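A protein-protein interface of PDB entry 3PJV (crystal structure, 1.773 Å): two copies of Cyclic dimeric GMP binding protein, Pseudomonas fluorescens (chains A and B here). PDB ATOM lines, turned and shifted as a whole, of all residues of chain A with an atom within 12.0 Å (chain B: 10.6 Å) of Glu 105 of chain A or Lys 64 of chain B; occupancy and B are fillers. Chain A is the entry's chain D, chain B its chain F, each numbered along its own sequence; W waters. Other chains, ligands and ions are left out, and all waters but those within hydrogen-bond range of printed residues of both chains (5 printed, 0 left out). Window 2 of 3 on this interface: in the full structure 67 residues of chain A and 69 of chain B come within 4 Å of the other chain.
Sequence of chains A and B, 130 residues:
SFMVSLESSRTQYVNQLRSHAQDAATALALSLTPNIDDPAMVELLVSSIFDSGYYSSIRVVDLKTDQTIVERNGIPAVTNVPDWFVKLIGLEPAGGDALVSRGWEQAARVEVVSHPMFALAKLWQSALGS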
ATOM      1  N   ALA A  98      39.056  25.884 -28.178  1.00  0.00           N
ATOM      2  CA  ALA A  98      39.065  27.305 -27.847  1.00  0.00           C
ATOM      3  C   ALA A  98      37.643  27.853 -27.888  1.00  0.00           C
ATOM      4  O   ALA A  98      36.796  27.343 -28.619  1.00  0.00           O
ATOM      5  CB  ALA A  98      39.965  28.070 -28.808  1.00  0.00           C
ATOM      6  N   LEU A  99      37.380  28.884 -27.094  1.00  0.00           N
ATOM      7  CA  LEU A  99      36.043  29.442 -26.995  1.00  0.00           C
ATOM      8  C   LEU A  99      35.877  30.654 -27.896  1.00  0.00           C
ATOM      9  O   LEU A  99      36.801  31.440 -28.069  1.00  0.00           O
ATOM     10  CB  LEU A  99      35.737  29.846 -25.552  1.00  0.00           C
ATOM     11  CG  LEU A  99      35.709  28.695 -24.545  1.00  0.00           C
ATOM     12  CD1 LEU A  99      35.251  29.181 -23.181  1.00  0.00           C
ATOM     13  CD2 LEU A  99      34.819  27.570 -25.043  1.00  0.00           C
ATOM     14  N   VAL A 100      34.688  30.779 -28.476  1.00  0.00           N
ATOM     15  CA  VAL A 100      34.297  31.967 -29.215  1.00  0.00           C
ATOM     16  C   VAL A 100      33.254  32.695 -28.376  1.00  0.00           C
ATOM     17  O   VAL A 100      32.268  32.096 -27.952  1.00  0.00           O
ATOM     18  CB  VAL A 100      33.648  31.619 -30.567  1.00  0.00           C
ATOM     19  CG1 VAL A 100      33.269  32.891 -31.317  1.00  0.00           C
ATOM     20  CG2 VAL A 100      34.568  30.728 -31.408  1.00  0.00           C
ATOM     21  N   SER A 101      33.473  33.984 -28.149  1.00  0.00           N
ATOM     22  CA  SER A 101      32.533  34.787 -27.383  1.00  0.00           C
ATOM     23  C   SER A 101      31.655  35.616 -28.297  1.00  0.00           C
ATOM     24  O   SER A 101      32.078  36.011 -29.383  1.00  0.00           O
ATOM     25  CB  SER A 101      33.278  35.692 -26.405  1.00  0.00           C
ATOM     26  OG  SER A 101      33.777  34.931 -25.317  1.00  0.00           O
ATOM     27  N   ARG A 102      30.418  35.834 -27.865  1.00  0.00           N
ATOM     28  CA  ARG A 102      29.509  36.759 -28.523  1.00  0.00           C
ATOM     29  C   ARG A 102      29.173  37.815 -27.482  1.00  0.00           C
ATOM     30  O   ARG A 102      28.383  37.567 -26.569  1.00  0.00           O
ATOM     31  CB  ARG A 102      28.238  36.046 -28.983  1.00  0.00           C
ATOM     32  CG  ARG A 102      27.300  36.913 -29.814  1.00  0.00           C
ATOM     33  CD  ARG A 102      25.902  36.300 -29.928  1.00  0.00           C
ATOM     34  NE  ARG A 102      25.904  34.975 -30.543  1.00  0.00           N
ATOM     35  CZ  ARG A 102      25.616  33.844 -29.902  1.00  0.00           C
ATOM     36  NH1 ARG A 102      25.645  32.690 -30.548  1.00  0.00           N
ATOM     37  NH2 ARG A 102      25.294  33.867 -28.614  1.00  0.00           N
ATOM     38  N   GLY A 103      29.791  38.981 -27.607  1.00  0.00           N
ATOM     39  CA  GLY A 103      29.694  39.988 -26.573  1.00  0.00           C
ATOM     40  C   GLY A 103      30.467  39.502 -25.365  1.00  0.00           C
ATOM     41  O   GLY A 103      31.673  39.269 -25.442  1.00  0.00           O
ATOM     42  N   TRP A 104      29.765  39.321 -24.252  1.00  0.00           N
ATOM     43  CA  TRP A 104      30.390  38.852 -23.022  1.00  0.00           C
ATOM     44  C   TRP A 104      30.060  37.398 -22.724  1.00  0.00           C
ATOM     45  O   TRP A 104      30.531  36.848 -21.736  1.00  0.00           O
ATOM     46  CB  TRP A 104      29.974  39.732 -21.849  1.00  0.00           C
ATOM     47  CG  TRP A 104      30.695  41.066 -21.844  1.00  0.00           C
ATOM     48  CD1 TRP A 104      31.887  41.347 -22.444  1.00  0.00           C
ATOM     49  CD2 TRP A 104      30.267  42.282 -21.210  1.00  0.00           C
ATOM     50  NE1 TRP A 104      32.234  42.668 -22.219  1.00  0.00           N
ATOM     51  CE2 TRP A 104      31.257  43.260 -21.468  1.00  0.00           C
ATOM     52  CE3 TRP A 104      29.147  42.641 -20.452  1.00  0.00           C
ATOM     53  CZ2 TRP A 104      31.155  44.564 -20.997  1.00  0.00           C
ATOM     54  CZ3 TRP A 104      29.049  43.937 -19.985  1.00  0.00           C
ATOM     55  CH2 TRP A 104      30.051  44.885 -20.259  1.00  0.00           C
ATOM     56  N   GLU A 105      29.239  36.781 -23.562  1.00  0.00           N
ATOM     57  CA  GLU A 105      28.855  35.397 -23.302  1.00  0.00           C
ATOM     58  C   GLU A 105      29.622  34.442 -24.206  1.00  0.00           C
ATOM     59  O   GLU A 105      29.833  34.736 -25.383  1.00  0.00           O
ATOM     60  CB  GLU A 105      27.355  35.194 -23.499  1.00  0.00           C
ATOM     61  CG  GLU A 105      26.921  33.759 -23.232  1.00  0.00           C
ATOM     62  CD  GLU A 105      25.429  33.548 -23.372  1.00  0.00           C
ATOM     63  OE1 GLU A 105      24.741  34.416 -23.962  1.00  0.00           O
ATOM     64  OE2 GLU A 105      24.945  32.504 -22.891  1.00  0.00           O
ATOM     65  N   GLN A 106      30.049  33.311 -23.659  1.00  0.00           N
ATOM     66  CA  GLN A 106      30.711  32.293 -24.476  1.00  0.00           C
ATOM     67  C   GLN A 106      29.658  31.657 -25.381  1.00  0.00           C
ATOM     68  O   GLN A 106      28.655  31.144 -24.897  1.00  0.00           O
ATOM     69  CB  GLN A 106      31.404  31.241 -23.603  1.00  0.00           C
ATOM     70  CG  GLN A 106      32.356  31.810 -22.541  1.00  0.00           C
ATOM     71  CD  GLN A 106      33.229  32.956 -23.051  1.00  0.00           C
ATOM     72  OE1 GLN A 106      33.054  34.115 -22.651  1.00  0.00           O
ATOM     73  NE2 GLN A 106      34.186  32.635 -23.922  1.00  0.00           N
ATOM     74  N   ALA A 107      29.883  31.719 -26.691  1.00  0.00           N
ATOM     75  CA  ALA A 107      28.863  31.376 -27.685  1.00  0.00           C
ATOM     76  C   ALA A 107      29.096  30.019 -28.358  1.00  0.00           C
ATOM     77  O   ALA A 107      28.151  29.312 -28.709  1.00  0.00           O
ATOM     78  CB  ALA A 107      28.772  32.475 -28.736  1.00  0.00           C
ATOM     79  N   ALA A 108      30.358  29.651 -28.536  1.00  0.00           N
ATOM     80  CA  ALA A 108      30.673  28.386 -29.199  1.00  0.00           C
ATOM     81  C   ALA A 108      32.053  27.891 -28.800  1.00  0.00           C
ATOM     82  O   ALA A 108      32.899  28.678 -28.369  1.00  0.00           O
ATOM     83  CB  ALA A 108      30.588  28.565 -30.716  1.00  0.00           C
ATOM     84  N   ARG A 109      32.264  26.585 -28.929  1.00  0.00           N
ATOM     85  CA  ARG A 109      33.564  25.974 -28.699  1.00  0.00           C
ATOM     86  C   ARG A 109      34.080  25.343 -29.997  1.00  0.00           C
ATOM     87  O   ARG A 109      33.356  24.599 -30.663  1.00  0.00           O
ATOM     88  CB  ARG A 109      33.485  24.910 -27.601  1.00  0.00           C
ATOM     89  CG  ARG A 109      34.798  24.196 -27.307  1.00  0.00           C
ATOM     90  CD  ARG A 109      34.660  23.188 -26.148  1.00  0.00           C
ATOM     91  NE  ARG A 109      33.783  22.071 -26.486  1.00  0.00           N
ATOM     92  CZ  ARG A 109      32.564  21.887 -25.983  1.00  0.00           C
ATOM     93  NH1 ARG A 109      32.055  22.751 -25.101  1.00  0.00           N
ATOM     94  NH2 ARG A 109      31.855  20.838 -26.368  1.00  0.00           N
ATOM     95  N   VAL A 110      35.320  25.671 -30.353  1.00  0.00           N
ATOM     96  CA  VAL A 110      35.990  25.080 -31.510  1.00  0.00           C
ATOM     97  C   VAL A 110      36.836  23.913 -31.026  1.00  0.00           C
ATOM     98  O   VAL A 110      37.677  24.079 -30.139  1.00  0.00           O
ATOM     99  CB  VAL A 110      36.925  26.094 -32.202  1.00  0.00           C
ATOM    100  CG1 VAL A 110      37.616  25.447 -33.399  1.00  0.00           C
ATOM    101  CG2 VAL A 110      36.156  27.330 -32.629  1.00  0.00           C
ATOM    102  N   GLU A 111      36.605  22.729 -31.590  1.00  0.00           N
ATOM    103  CA  GLU A 111      37.364  21.544 -31.220  1.00  0.00           C
ATOM    104  C   GLU A 111      38.178  21.056 -32.412  1.00  0.00           C
ATOM    105  O   GLU A 111      37.631  20.849 -33.485  1.00  0.00           O
ATOM    106  CB  GLU A 111      36.421  20.429 -30.773  1.00  0.00           C
ATOM    107  CG  GLU A 111      35.487  20.861 -29.649  1.00  0.00           C
ATOM    108  CD  GLU A 111      34.515  19.766 -29.239  1.00  0.00           C
ATOM    109  OE1 GLU A 111      34.242  18.860 -30.056  1.00  0.00           O
ATOM    110  OE2 GLU A 111      34.033  19.815 -28.090  1.00  0.00           O
ATOM    111  N   THR B  33      35.203  34.883 -34.534  1.00  0.00           N
ATOM    112  CA  THR B  33      34.615  35.803 -33.570  1.00  0.00           C
ATOM    113  C   THR B  33      33.734  36.879 -34.209  1.00  0.00           C
ATOM    114  O   THR B  33      32.586  37.049 -33.810  1.00  0.00           O
ATOM    115  CB  THR B  33      35.682  36.397 -32.636  1.00  0.00           C
ATOM    116  OG1 THR B  33      36.203  35.344 -31.815  1.00  0.00           O
ATOM    117  CG2 THR B  33      35.076  37.466 -31.741  1.00  0.00           C
ATOM    118  N   ILE B  36      30.371  35.038 -35.971  1.00  0.00           N
ATOM    119  CA  ILE B  36      29.652  33.961 -35.299  1.00  0.00           C
ATOM    120  C   ILE B  36      28.151  33.923 -35.610  1.00  0.00           C
ATOM    121  O   ILE B  36      27.529  32.867 -35.525  1.00  0.00           O
ATOM    122  CB  ILE B  36      29.894  33.971 -33.769  1.00  0.00           C
ATOM    123  CG1 ILE B  36      29.637  32.579 -33.178  1.00  0.00           C
ATOM    124  CG2 ILE B  36      29.053  35.038 -33.102  1.00  0.00           C
ATOM    125  CD1 ILE B  36      30.582  31.512 -33.681  1.00  0.00           C
ATOM    126  N   ASP B  37      27.574  35.057 -35.992  1.00  0.00           N
ATOM    127  CA  ASP B  37      26.141  35.106 -36.296  1.00  0.00           C
ATOM    128  C   ASP B  37      25.843  34.899 -37.782  1.00  0.00           C
ATOM    129  O   ASP B  37      24.701  35.053 -38.222  1.00  0.00           O
ATOM    130  CB  ASP B  37      25.531  36.432 -35.831  1.00  0.00           C
ATOM    131  CG  ASP B  37      25.532  36.577 -34.320  1.00  0.00           C
ATOM    132  OD1 ASP B  37      25.330  35.563 -33.621  1.00  0.00           O
ATOM    133  OD2 ASP B  37      25.741  37.709 -33.835  1.00  0.00           O
ATOM    134  N   VAL B  60      32.601  22.656 -34.448  1.00  0.00           N
ATOM    135  CA  VAL B  60      32.172  23.842 -33.716  1.00  0.00           C
ATOM    136  C   VAL B  60      30.851  23.534 -33.030  1.00  0.00           C
ATOM    137  O   VAL B  60      29.892  23.105 -33.677  1.00  0.00           O
ATOM    138  CB  VAL B  60      32.008  25.043 -34.663  1.00  0.00           C
ATOM    139  CG1 VAL B  60      31.548  26.266 -33.881  1.00  0.00           C
ATOM    140  CG2 VAL B  60      33.327  25.315 -35.384  1.00  0.00           C
ATOM    141  N   VAL B  61      30.816  23.712 -31.709  1.00  0.00           N
ATOM    142  CA  VAL B  61      29.637  23.403 -30.912  1.00  0.00           C
ATOM    143  C   VAL B  61      28.982  24.690 -30.401  1.00  0.00           C
ATOM    144  O   VAL B  61      29.659  25.556 -29.858  1.00  0.00           O
ATOM    145  CB  VAL B  61      30.018  22.532 -29.695  1.00  0.00           C
ATOM    146  CG1 VAL B  61      28.794  22.240 -28.822  1.00  0.00           C
ATOM    147  CG2 VAL B  61      30.676  21.231 -30.149  1.00  0.00           C
ATOM    148  N   ASP B  62      27.671  24.804 -30.590  1.00  0.00           N
ATOM    149  CA  ASP B  62      26.882  25.919 -30.051  1.00  0.00           C
ATOM    150  C   ASP B  62      26.697  25.708 -28.549  1.00  0.00           C
ATOM    151  O   ASP B  62      26.086  24.727 -28.128  1.00  0.00           O
ATOM    152  CB  ASP B  62      25.517  25.972 -30.749  1.00  0.00           C
ATOM    153  CG  ASP B  62      24.676  27.167 -30.330  1.00  0.00           C
ATOM    154  OD1 ASP B  62      24.897  27.718 -29.230  1.00  0.00           O
ATOM    155  OD2 ASP B  62      23.776  27.546 -31.108  1.00  0.00           O
ATOM    156  N   LEU B  63      27.232  26.625 -27.748  1.00  0.00           N
ATOM    157  CA  LEU B  63      27.236  26.468 -26.295  1.00  0.00           C
ATOM    158  C   LEU B  63      25.876  26.770 -25.681  1.00  0.00           C
ATOM    159  O   LEU B  63      25.571  26.320 -24.578  1.00  0.00           O
ATOM    160  CB  LEU B  63      28.317  27.350 -25.665  1.00  0.00           C
ATOM    161  CG  LEU B  63      29.747  26.899 -25.964  1.00  0.00           C
ATOM    162  CD1 LEU B  63      30.767  27.841 -25.349  1.00  0.00           C
ATOM    163  CD2 LEU B  63      29.956  25.477 -25.466  1.00  0.00           C
ATOM    164  N   LYS B  64      25.057  27.525 -26.405  1.00  0.00           N
ATOM    165  CA  LYS B  64      23.723  27.864 -25.930  1.00  0.00           C
ATOM    166  C   LYS B  64      22.812  26.633 -25.985  1.00  0.00           C
ATOM    167  O   LYS B  64      21.906  26.485 -25.164  1.00  0.00           O
ATOM    168  CB  LYS B  64      23.139  29.004 -26.766  1.00  0.00           C
ATOM    169  CG  LYS B  64      22.047  29.789 -26.067  1.00  0.00           C
ATOM    170  CD  LYS B  64      22.595  30.566 -24.880  1.00  0.00           C
ATOM    171  CE  LYS B  64      21.473  31.236 -24.101  1.00  0.00           C
ATOM    172  NZ  LYS B  64      21.983  31.987 -22.922  1.00  0.00           N
ATOM    173  N   THR B  65      23.071  25.746 -26.944  1.00  0.00           N
ATOM    174  CA  THR B  65      22.266  24.537 -27.131  1.00  0.00           C
ATOM    175  C   THR B  65      23.041  23.243 -26.860  1.00  0.00           C
ATOM    176  O   THR B  65      22.449  22.162 -26.753  1.00  0.00           O
ATOM    177  CB  THR B  65      21.741  24.451 -28.563  1.00  0.00           C
ATOM    178  OG1 THR B  65      22.857  24.362 -29.463  1.00  0.00           O
ATOM    179  CG2 THR B  65      20.914  25.683 -28.899  1.00  0.00           C
ATOM    180  N   ASP B  66      24.360  23.354 -26.760  1.00  0.00           N
ATOM    181  CA  ASP B  66      25.239  22.190 -26.624  1.00  0.00           C
ATOM    182  C   ASP B  66      25.113  21.228 -27.808  1.00  0.00           C
ATOM    183  O   ASP B  66      25.223  20.013 -27.645  1.00  0.00           O
ATOM    184  CB  ASP B  66      24.983  21.446 -25.308  1.00  0.00           C
ATOM    185  CG  ASP B  66      26.089  20.461 -24.976  1.00  0.00           C
ATOM    186  OD1 ASP B  66      25.806  19.432 -24.327  1.00  0.00           O
ATOM    187  OD2 ASP B  66      27.247  20.719 -25.374  1.00  0.00           O
ATOM    188  N   GLN B  67      24.894  21.776 -28.998  1.00  0.00           N
ATOM    189  CA  GLN B  67      24.762  20.957 -30.199  1.00  0.00           C
ATOM    190  C   GLN B  67      25.704  21.415 -31.309  1.00  0.00           C
ATOM    191  O   GLN B  67      26.020  22.597 -31.415  1.00  0.00           O
ATOM    192  CB  GLN B  67      23.322  20.972 -30.693  1.00  0.00           C
ATOM    193  CG  GLN B  67      22.400  20.072 -29.887  1.00  0.00           C
ATOM    194  CD  GLN B  67      20.979  20.581 -29.864  1.00  0.00           C
ATOM    195  OE1 GLN B  67      20.188  20.220 -28.990  1.00  0.00           O
ATOM    196  NE2 GLN B  67      20.644  21.438 -30.824  1.00  0.00           N
ATOM    197  N   THR B  68      26.132  20.470 -32.140  1.00  0.00           N
ATOM    198  CA  THR B  68      27.096  20.760 -33.203  1.00  0.00           C
ATOM    199  C   THR B  68      26.552  21.753 -34.226  1.00  0.00           C
ATOM    200  O   THR B  68      25.440  21.596 -34.724  1.00  0.00           O
ATOM    201  CB  THR B  68      27.513  19.472 -33.927  1.00  0.00           C
ATOM    202  OG1 THR B  68      28.109  18.570 -32.988  1.00  0.00           O
ATOM    203  CG2 THR B  68      28.514  19.781 -35.042  1.00  0.00           C
ATOM    204  N   ILE B  69      27.342  22.782 -34.528  1.00  0.00           N
ATOM    205  CA  ILE B  69      27.005  23.763 -35.558  1.00  0.00           C
ATOM    206  C   ILE B  69      27.525  23.298 -36.914  1.00  0.00           C
ATOM    207  O   ILE B  69      26.764  23.165 -37.874  1.00  0.00           O
ATOM    208  CB  ILE B  69      27.668  25.132 -35.285  1.00  0.00           C
ATOM    209  CG1 ILE B  69      27.063  25.813 -34.062  1.00  0.00           C
ATOM    210  CG2 ILE B  69      27.532  26.043 -36.497  1.00  0.00           C
ATOM    211  CD1 ILE B  69      27.702  27.166 -33.763  1.00  0.00           C
HETATM  212  O   HOH W   1      25.628  30.170 -29.344  1.00  0.00           O
HETATM  213  O   HOH W   2      35.899  35.312 -29.019  1.00  0.00           O
HETATM  214  O   HOH W   3      29.853  19.428 -25.297  1.00  0.00           O
HETATM  215  O   HOH W   4      29.383  21.915 -23.808  1.00  0.00           O
HETATM  216  O   HOH W   5      31.401  37.568 -31.538  1.00  0.00           O
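NE of Arg 102 of chain A lies within salt-bridge range of OD1 of Asp 37 of chain B. OE2 of Glu 105 of chain A lies within salt-bridge range of NZ of Lys 64 of chain B, at 3.0 Å. The backbone NH (N) of Leu 63 of chain B lies within hydrogen-bond range of the backbone carbonyl oxygen (O) of Ala 107 of chain A (3.0 Å). The backbone NH (N) of Val 61 of chain B lies within hydrogen-bond range of the backbone carbonyl oxygen (O) of Arg 109 of chain A (2.9 Å).
O of Val 100 of chain A lies within hydrogen-bond range of N of Ala 107 of chain A, 2.7 Å away. N of Val 100 of chain A sits at hydrogen-bond distance from O of Ala 108 of chain A, 2.8 Å away. NE of Arg 109 of chain A is in salt-bridge range of OE2 of Glu 111 of chain A. The backbone carbonyl oxygen of Val 60 of chain B lies within hydrogen-bond range of the backbone NH of Ile 69 of chain B (2.7 Å). N of Lys 64 of chain B is in hydrogen-bond range of OD1 of Asp 62 of chain B (2.8 Å). The backbone carbonyl oxygen (O) of Gln 67 of chain B sits at hydrogen-bond distance from the backbone NH (N) of Asp 62 of chain B (2.9 Å).
Among the printed residues, pairs that only touch across the chains: Ala 108 of chain A with Val 61 of chain B (3.1 Å), Arg 109 of chain A with Val 60 of chain B (3.4 Å), Arg 109 of chain A with Leu 63 of chain B (3.5 Å), Ala 107 of chain A with Asp 62 of chain B (3.7 Å), Ala 108 of chain A with Leu 63 of chain B (3.7 Å), Val 100 of chain A with Ile 36 of chain B (3.8 Å), Val 100 of chain A with Thr 33 of chain B (3.9 Å) and Gln 106 of chain A with Leu 63 of chain B (3.9 Å).
Glu 105 of chain A touches just one residue of chain B: Lys 64. Lys 64 of chain B touches just one residue of chain A: Glu 105. No residue of chain B comes within 4 Å of Ser 101 of chain A. No residue of chain B comes within 4 Å of Gly 103 of chain A. Of chain B, only Leu 63 comes within 4 Å of Gln 106 of chain A. Ala 107 of chain A touches just these residues of chain B: Asp 62 and Leu 63. No residue of chain A comes within 4 Å of Thr 65 of chain B. No residue of chain A comes within 4 Å of Gln 67 of chain B. Of the printed residues of chain B, Val 100 of chain A touches Thr 33 (3.9 Å) and Ile 36 (3.8 Å). Of the printed residues of chain A, Val 60 of chain B touches Arg 109 (3.4 Å). Of the printed residues of chain A, Asp 37 of chain B touches Arg 102 (3.2 Å). Thr 68 of chain B touches none of the printed residues of chain A. The nearest residue of chain B that does not touch Glu 105 of chain A is Leu 63 of chain B (6.4 Å). The nearest printed residue of chain A that does not touch Ile 36 of chain B is Arg 102 of chain A (4.1 Å).
Of the 14 printed residues of chain A, 7 touch a printed residue of chain B. Hydrophobic or aromatic side chains of chain A that line the printed part of chain B: Val 100 and Ala 108. Along chain A the printed residues that touch a printed residue of chain B span positions 100 to 109. Among the printed residues, 12 pairs touch across the chains. Among the printed residues, Asp or Glu carboxylates within 4 Å of a Lys or Arg side-chain nitrogen of the other chain: Arg 102 of chain A with Asp 37 of chain B and Glu 105 of chain A with Lys 64 of chain B.
No position is printed for both chains.
Water W1 lies within hydrogen-bond range of OD1 of Asp 62 of chain B, O of Ala 107 of chain A and NH1 of Arg 102 of chain A. Water W5 bridges O of Thr 33 of chain B and O of Ser 101 of chain A. Water W3 lies within hydrogen-bond range of the guanidinium group of Arg 109 of chain A (2.7 Å) and the side-chain carboxylate of Asp 66 of chain B (2.9 Å). Water W2 bridges the side-chain hydroxyl (OG1) of Thr 33 of chain B (2.8 Å) and the backbone NH (N) of Ser 101 of chain A (2.9 Å). Water W4 bridges the side-chain carboxylate of Asp 66 of chain B (2.9 Å) and the guanidinium group of Arg 109 of chain A (3.1 Å).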
